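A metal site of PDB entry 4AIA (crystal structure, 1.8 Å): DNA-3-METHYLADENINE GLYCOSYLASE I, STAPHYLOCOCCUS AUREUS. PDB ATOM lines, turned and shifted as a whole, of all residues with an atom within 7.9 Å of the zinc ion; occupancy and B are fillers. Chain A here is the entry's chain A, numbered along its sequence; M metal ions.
A ring nitrogen (NE2) of His 177 lies within hydrogen-bond range of the backbone carbonyl oxygen (O) of Trp 23 (2.8 Å). O of His 177 lies within hydrogen-bond range of NZ of Lys 184 (3.2 Å). The side-chain amide nitrogen of Gln 25 lies within hydrogen-bond range of a ring nitrogen (NE2) of His 177, 3.4 Å away. N of His 177 sits at hydrogen-bond distance from OD1 of Asp 175 (2.9 Å). The side-chain sulfur of Cys 6 lies close to the backbone NH of Leu 178 (3.3 Å). The backbone carbonyl oxygen (O) of Cys 6 sits at hydrogen-bond distance from the guanidinium group (NH2) of Arg 137. SG of Cys 181 lies close to N of Ser 183, at 3.3 Å.
Within 4 Å of the zinc ion: Cys 6, His 19, His 177 and Cys 181. Along chain A the residues within 4 Å of the zinc ion span positions 6 to 181.
The zinc ion is bound by a ring nitrogen (NE2) of His 19 (2.0 Å). ND1 of His 177 binds the zinc ion. SG of Cys 6 binds the zinc ion. The zinc ion is bound by SG of Cys 181.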
ATOM      1  N   ALA A   2      22.708   9.363 -11.747  1.00  0.00           N
ATOM      2  CA  ALA A   2      22.871  10.341 -10.689  1.00  0.00           C
ATOM      3  C   ALA A   2      23.927   9.929  -9.661  1.00  0.00           C
ATOM      4  O   ALA A   2      24.718  10.766  -9.211  1.00  0.00           O
ATOM      5  CB  ALA A   2      21.524  10.610 -10.005  1.00  0.00           C
ATOM      6  N   MET A   3      23.968   8.645  -9.296  1.00  0.00           N
ATOM      7  CA  MET A   3      24.944   8.277  -8.242  1.00  0.00           C
ATOM      8  C   MET A   3      26.371   8.466  -8.737  1.00  0.00           C
ATOM      9  O   MET A   3      27.227   8.920  -7.993  1.00  0.00           O
ATOM     10  CB  MET A   3      24.772   6.842  -7.760  1.00  0.00           C
ATOM     11  CG  MET A   3      25.346   6.673  -6.370  1.00  0.00           C
ATOM     12  SD  MET A   3      25.530   4.961  -5.872  1.00  0.00           S
ATOM     13  CE  MET A   3      26.058   5.175  -4.182  1.00  0.00           C
ATOM     14  N   ASN A   4      26.610   8.096  -9.995  1.00  0.00           N
ATOM     15  CA  ASN A   4      27.920   8.302 -10.593  1.00  0.00           C
ATOM     16  C   ASN A   4      28.356   9.786 -10.567  1.00  0.00           C
ATOM     17  O   ASN A   4      29.505  10.113 -10.228  1.00  0.00           O
ATOM     18  CB  ASN A   4      27.917   7.795 -12.020  1.00  0.00           C
ATOM     19  CG  ASN A   4      29.283   7.848 -12.640  1.00  0.00           C
ATOM     20  OD1 ASN A   4      29.761   8.929 -13.011  1.00  0.00           O
ATOM     21  ND2 ASN A   4      29.952   6.723 -12.672  1.00  0.00           N
ATOM     22  N   GLU A   5      27.424  10.657 -10.923  1.00  0.00           N
ATOM     23  CA  GLU A   5      27.701  12.104 -10.938  1.00  0.00           C
ATOM     24  C   GLU A   5      27.955  12.618  -9.520  1.00  0.00           C
ATOM     25  O   GLU A   5      28.830  13.483  -9.299  1.00  0.00           O
ATOM     26  CB  GLU A   5      26.541  12.857 -11.568  1.00  0.00           C
ATOM     27  CG  GLU A   5      26.942  14.288 -11.940  1.00  0.00           C
ATOM     28  CD  GLU A   5      25.767  15.132 -12.429  1.00  0.00           C
ATOM     29  OE1 GLU A   5      24.690  14.559 -12.736  1.00  0.00           O
ATOM     30  OE2 GLU A   5      25.934  16.366 -12.510  1.00  0.00           O
ATOM     31  N   CYS A   6      27.201  12.077  -8.570  1.00  0.00           N
ATOM     32  CA  CYS A   6      27.288  12.560  -7.194  1.00  0.00           C
ATOM     33  C   CYS A   6      28.548  12.071  -6.510  1.00  0.00           C
ATOM     34  O   CYS A   6      29.171  12.825  -5.763  1.00  0.00           O
ATOM     35  CB  CYS A   6      26.039  12.142  -6.417  1.00  0.00           C
ATOM     36  SG  CYS A   6      25.929  12.903  -4.766  1.00  0.00           S
ATOM     37  N   ALA A   7      28.922  10.824  -6.785  1.00  0.00           N
ATOM     38  CA  ALA A   7      29.945  10.107  -6.036  1.00  0.00           C
ATOM     39  C   ALA A   7      31.311  10.130  -6.710  1.00  0.00           C
ATOM     40  O   ALA A   7      32.068   9.158  -6.607  1.00  0.00           O
ATOM     41  CB  ALA A   7      29.493   8.664  -5.778  1.00  0.00           C
ATOM     42  N   PHE A   8      31.634  11.246  -7.361  1.00  0.00           N
ATOM     43  CA  PHE A   8      32.973  11.519  -7.922  1.00  0.00           C
ATOM     44  C   PHE A   8      33.392  10.463  -8.952  1.00  0.00           C
ATOM     45  O   PHE A   8      34.565  10.100  -9.079  1.00  0.00           O
ATOM     46  CB  PHE A   8      33.979  11.739  -6.777  1.00  0.00           C
ATOM     47  CG  PHE A   8      33.453  12.663  -5.694  1.00  0.00           C
ATOM     48  CD1 PHE A   8      33.491  14.040  -5.851  1.00  0.00           C
ATOM     49  CD2 PHE A   8      32.820  12.140  -4.560  1.00  0.00           C
ATOM     50  CE1 PHE A   8      32.955  14.890  -4.887  1.00  0.00           C
ATOM     51  CE2 PHE A   8      32.283  12.973  -3.594  1.00  0.00           C
ATOM     52  CZ  PHE A   8      32.354  14.359  -3.756  1.00  0.00           C
ATOM     53  N   HIS A  19      30.179   6.637   0.417  1.00  0.00           N
ATOM     54  CA  HIS A  19      29.184   7.593  -0.115  1.00  0.00           C
ATOM     55  C   HIS A  19      27.793   7.352   0.440  1.00  0.00           C
ATOM     56  O   HIS A  19      27.067   8.292   0.797  1.00  0.00           O
ATOM     57  CB  HIS A  19      29.112   7.494  -1.666  1.00  0.00           C
ATOM     58  CG  HIS A  19      28.364   8.642  -2.303  1.00  0.00           C
ATOM     59  ND1 HIS A  19      28.950   9.853  -2.496  1.00  0.00           N
ATOM     60  CD2 HIS A  19      27.046   8.756  -2.730  1.00  0.00           C
ATOM     61  CE1 HIS A  19      28.061  10.701  -3.041  1.00  0.00           C
ATOM     62  NE2 HIS A  19      26.881  10.046  -3.182  1.00  0.00           N
ATOM     63  N   ASP A  20      27.416   6.081   0.544  1.00  0.00           N
ATOM     64  CA  ASP A  20      26.045   5.723   0.946  1.00  0.00           C
ATOM     65  C   ASP A  20      25.845   5.775   2.450  1.00  0.00           C
ATOM     66  O   ASP A  20      24.759   6.099   2.923  1.00  0.00           O
ATOM     67  CB  ASP A  20      25.619   4.354   0.401  1.00  0.00           C
ATOM     68  CG  ASP A  20      24.134   4.050   0.674  1.00  0.00           C
ATOM     69  OD1 ASP A  20      23.273   4.912   0.368  1.00  0.00           O
ATOM     70  OD2 ASP A  20      23.829   2.972   1.232  1.00  0.00           O
ATOM     71  N   TRP A  23      29.208   9.657   3.955  1.00  0.00           N
ATOM     72  CA  TRP A  23      29.294  11.003   3.387  1.00  0.00           C
ATOM     73  C   TRP A  23      27.934  11.678   3.323  1.00  0.00           C
ATOM     74  O   TRP A  23      26.967  11.134   2.762  1.00  0.00           O
ATOM     75  CB  TRP A  23      29.947  10.937   2.012  1.00  0.00           C
ATOM     76  CG  TRP A  23      30.388  12.275   1.497  1.00  0.00           C
ATOM     77  CD1 TRP A  23      31.515  13.019   1.883  1.00  0.00           C
ATOM     78  CD2 TRP A  23      29.735  13.071   0.464  1.00  0.00           C
ATOM     79  NE1 TRP A  23      31.587  14.192   1.189  1.00  0.00           N
ATOM     80  CE2 TRP A  23      30.557  14.270   0.295  1.00  0.00           C
ATOM     81  CE3 TRP A  23      28.599  12.907  -0.328  1.00  0.00           C
ATOM     82  CZ2 TRP A  23      30.224  15.267  -0.622  1.00  0.00           C
ATOM     83  CZ3 TRP A  23      28.270  13.908  -1.254  1.00  0.00           C
ATOM     84  CH2 TRP A  23      29.078  15.058  -1.407  1.00  0.00           C
ATOM     85  N   GLN A  25      25.748  11.990   5.629  1.00  0.00           N
ATOM     86  CA  GLN A  25      24.752  11.406   6.498  1.00  0.00           C
ATOM     87  C   GLN A  25      24.963  11.995   7.890  1.00  0.00           C
ATOM     88  O   GLN A  25      26.034  11.813   8.477  1.00  0.00           O
ATOM     89  CB  GLN A  25      24.845   9.860   6.461  1.00  0.00           C
ATOM     90  CG  GLN A  25      25.127   9.274   5.054  1.00  0.00           C
ATOM     91  CD  GLN A  25      24.020   9.498   4.035  1.00  0.00           C
ATOM     92  OE1 GLN A  25      22.856   9.711   4.389  1.00  0.00           O
ATOM     93  NE2 GLN A  25      24.364   9.430   2.733  1.00  0.00           N
ATOM     94  N   ARG A 137      28.670  22.438  -7.406  1.00  0.00           N
ATOM     95  CA  ARG A 137      29.347  22.349  -6.110  1.00  0.00           C
ATOM     96  C   ARG A 137      30.398  23.397  -5.883  1.00  0.00           C
ATOM     97  O   ARG A 137      31.192  23.670  -6.767  1.00  0.00           O
ATOM     98  CB  ARG A 137      29.969  20.973  -5.945  1.00  0.00           C
ATOM     99  CG  ARG A 137      28.917  19.887  -5.815  1.00  0.00           C
ATOM    100  CD  ARG A 137      29.492  18.778  -4.975  1.00  0.00           C
ATOM    101  NE  ARG A 137      28.585  17.615  -4.787  1.00  0.00           N
ATOM    102  CZ  ARG A 137      28.833  16.391  -5.252  1.00  0.00           C
ATOM    103  NH1 ARG A 137      29.932  16.149  -5.967  1.00  0.00           N
ATOM    104  NH2 ARG A 137      27.985  15.411  -4.987  1.00  0.00           N
ATOM    105  N   ASP A 175      24.597  18.787   3.442  1.00  0.00           N
ATOM    106  CA  ASP A 175      24.220  17.705   2.502  1.00  0.00           C
ATOM    107  C   ASP A 175      24.570  18.201   1.096  1.00  0.00           C
ATOM    108  O   ASP A 175      23.871  19.060   0.541  1.00  0.00           O
ATOM    109  CB  ASP A 175      22.716  17.410   2.625  1.00  0.00           C
ATOM    110  CG  ASP A 175      22.197  16.440   1.550  1.00  0.00           C
ATOM    111  OD1 ASP A 175      23.001  15.886   0.767  1.00  0.00           O
ATOM    112  OD2 ASP A 175      20.974  16.223   1.471  1.00  0.00           O
ATOM    113  N   ALA A 176      25.658  17.659   0.565  1.00  0.00           N
ATOM    114  CA  ALA A 176      26.129  17.969  -0.781  1.00  0.00           C
ATOM    115  C   ALA A 176      25.782  16.893  -1.827  1.00  0.00           C
ATOM    116  O   ALA A 176      26.278  16.962  -2.964  1.00  0.00           O
ATOM    117  CB  ALA A 176      27.632  18.260  -0.760  1.00  0.00           C
ATOM    118  N   HIS A 177      24.890  15.954  -1.497  1.00  0.00           N
ATOM    119  CA  HIS A 177      24.434  15.012  -2.505  1.00  0.00           C
ATOM    120  C   HIS A 177      23.563  15.714  -3.514  1.00  0.00           C
ATOM    121  O   HIS A 177      22.797  16.605  -3.188  1.00  0.00           O
ATOM    122  CB  HIS A 177      23.600  13.870  -1.883  1.00  0.00           C
ATOM    123  CG  HIS A 177      24.395  12.904  -1.052  1.00  0.00           C
ATOM    124  ND1 HIS A 177      24.940  11.776  -1.579  1.00  0.00           N
ATOM    125  CD2 HIS A 177      24.702  12.882   0.315  1.00  0.00           C
ATOM    126  CE1 HIS A 177      25.570  11.095  -0.616  1.00  0.00           C
ATOM    127  NE2 HIS A 177      25.405  11.764   0.558  1.00  0.00           N
ATOM    128  N   LEU A 178      23.650  15.267  -4.758  1.00  0.00           N
ATOM    129  CA  LEU A 178      22.759  15.771  -5.810  1.00  0.00           C
ATOM    130  C   LEU A 178      21.309  15.350  -5.562  1.00  0.00           C
ATOM    131  O   LEU A 178      21.046  14.277  -4.995  1.00  0.00           O
ATOM    132  CB  LEU A 178      23.236  15.250  -7.169  1.00  0.00           C
ATOM    133  CG  LEU A 178      24.735  15.509  -7.424  1.00  0.00           C
ATOM    134  CD1 LEU A 178      25.044  15.132  -8.875  1.00  0.00           C
ATOM    135  CD2 LEU A 178      25.143  16.956  -7.174  1.00  0.00           C
ATOM    136  N   LYS A 179      20.397  16.170  -6.072  1.00  0.00           N
ATOM    137  CA  LYS A 179      18.968  15.965  -5.819  1.00  0.00           C
ATOM    138  C   LYS A 179      18.530  14.531  -6.160  1.00  0.00           C
ATOM    139  O   LYS A 179      17.755  13.934  -5.409  1.00  0.00           O
ATOM    140  CB  LYS A 179      18.116  17.003  -6.537  1.00  0.00           C
ATOM    141  CG  LYS A 179      16.700  17.125  -5.977  1.00  0.00           C
ATOM    142  CD  LYS A 179      15.919  18.265  -6.609  1.00  0.00           C
ATOM    143  CE  LYS A 179      15.643  17.978  -8.082  1.00  0.00           C
ATOM    144  NZ  LYS A 179      14.184  18.124  -8.382  1.00  0.00           N
ATOM    145  N   ASP A 180      19.041  13.985  -7.262  1.00  0.00           N
ATOM    146  CA  ASP A 180      18.588  12.645  -7.693  1.00  0.00           C
ATOM    147  C   ASP A 180      19.480  11.485  -7.244  1.00  0.00           C
ATOM    148  O   ASP A 180      19.281  10.346  -7.673  1.00  0.00           O
ATOM    149  CB  ASP A 180      18.441  12.595  -9.213  1.00  0.00           C
ATOM    150  CG  ASP A 180      17.325  13.480  -9.715  1.00  0.00           C
ATOM    151  OD1 ASP A 180      16.383  13.787  -8.969  1.00  0.00           O
ATOM    152  OD2 ASP A 180      17.390  13.845 -10.890  1.00  0.00           O
ATOM    153  N   CYS A 181      20.464  11.778  -6.386  1.00  0.00           N
ATOM    154  CA  CYS A 181      21.349  10.706  -5.940  1.00  0.00           C
ATOM    155  C   CYS A 181      20.548   9.744  -5.058  1.00  0.00           C
ATOM    156  O   CYS A 181      19.889  10.189  -4.113  1.00  0.00           O
ATOM    157  CB  CYS A 181      22.533  11.245  -5.153  1.00  0.00           C
ATOM    158  SG  CYS A 181      23.606   9.925  -4.517  1.00  0.00           S
ATOM    159  N   PRO A 182      20.657   8.441  -5.309  1.00  0.00           N
ATOM    160  CA  PRO A 182      19.934   7.496  -4.482  1.00  0.00           C
ATOM    161  C   PRO A 182      20.385   7.461  -3.023  1.00  0.00           C
ATOM    162  O   PRO A 182      19.661   6.878  -2.193  1.00  0.00           O
ATOM    163  CB  PRO A 182      20.180   6.145  -5.188  1.00  0.00           C
ATOM    164  CG  PRO A 182      21.483   6.312  -5.859  1.00  0.00           C
ATOM    165  CD  PRO A 182      21.465   7.752  -6.348  1.00  0.00           C
ATOM    166  N   SER A 183      21.537   8.077  -2.708  1.00  0.00           N
ATOM    167  CA  SER A 183      22.083   8.128  -1.343  1.00  0.00           C
ATOM    168  C   SER A 183      21.756   9.441  -0.609  1.00  0.00           C
ATOM    169  O   SER A 183      22.147   9.620   0.564  1.00  0.00           O
ATOM    170  CB  SER A 183      23.609   7.878  -1.340  1.00  0.00           C
ATOM    171  OG  SER A 183      23.911   6.545  -1.768  1.00  0.00           O
ATOM    172  N   LYS A 184      21.040  10.345  -1.268  1.00  0.00           N
ATOM    173  CA  LYS A 184      20.720  11.637  -0.639  1.00  0.00           C
ATOM    174  C   LYS A 184      19.849  11.423   0.598  1.00  0.00           C
ATOM    175  O   LYS A 184      18.815  10.726   0.510  1.00  0.00           O
ATOM    176  CB  LYS A 184      20.061  12.597  -1.621  1.00  0.00           C
ATOM    177  CG  LYS A 184      19.886  14.004  -1.024  1.00  0.00           C
ATOM    178  CD  LYS A 184      19.279  14.983  -2.022  1.00  0.00           C
ATOM    179  CE  LYS A 184      19.071  16.348  -1.365  1.00  0.00           C
ATOM    180  NZ  LYS A 184      20.382  17.004  -1.118  1.00  0.00           N
ATOM    181  N   PRO A 185      20.278  11.949   1.757  1.00  0.00           N
ATOM    182  CA  PRO A 185      19.466  11.760   2.947  1.00  0.00           C
ATOM    183  C   PRO A 185      18.168  12.559   2.880  1.00  0.00           C
ATOM    184  O   PRO A 185      18.087  13.577   2.182  1.00  0.00           O
ATOM    185  CB  PRO A 185      20.365  12.278   4.087  1.00  0.00           C
ATOM    186  CG  PRO A 185      21.336  13.192   3.436  1.00  0.00           C
ATOM    187  CD  PRO A 185      21.529  12.688   2.036  1.00  0.00           C
HETATM  188 ZN    ZN M   1      25.253  11.140  -3.500  1.00  0.00          ZN
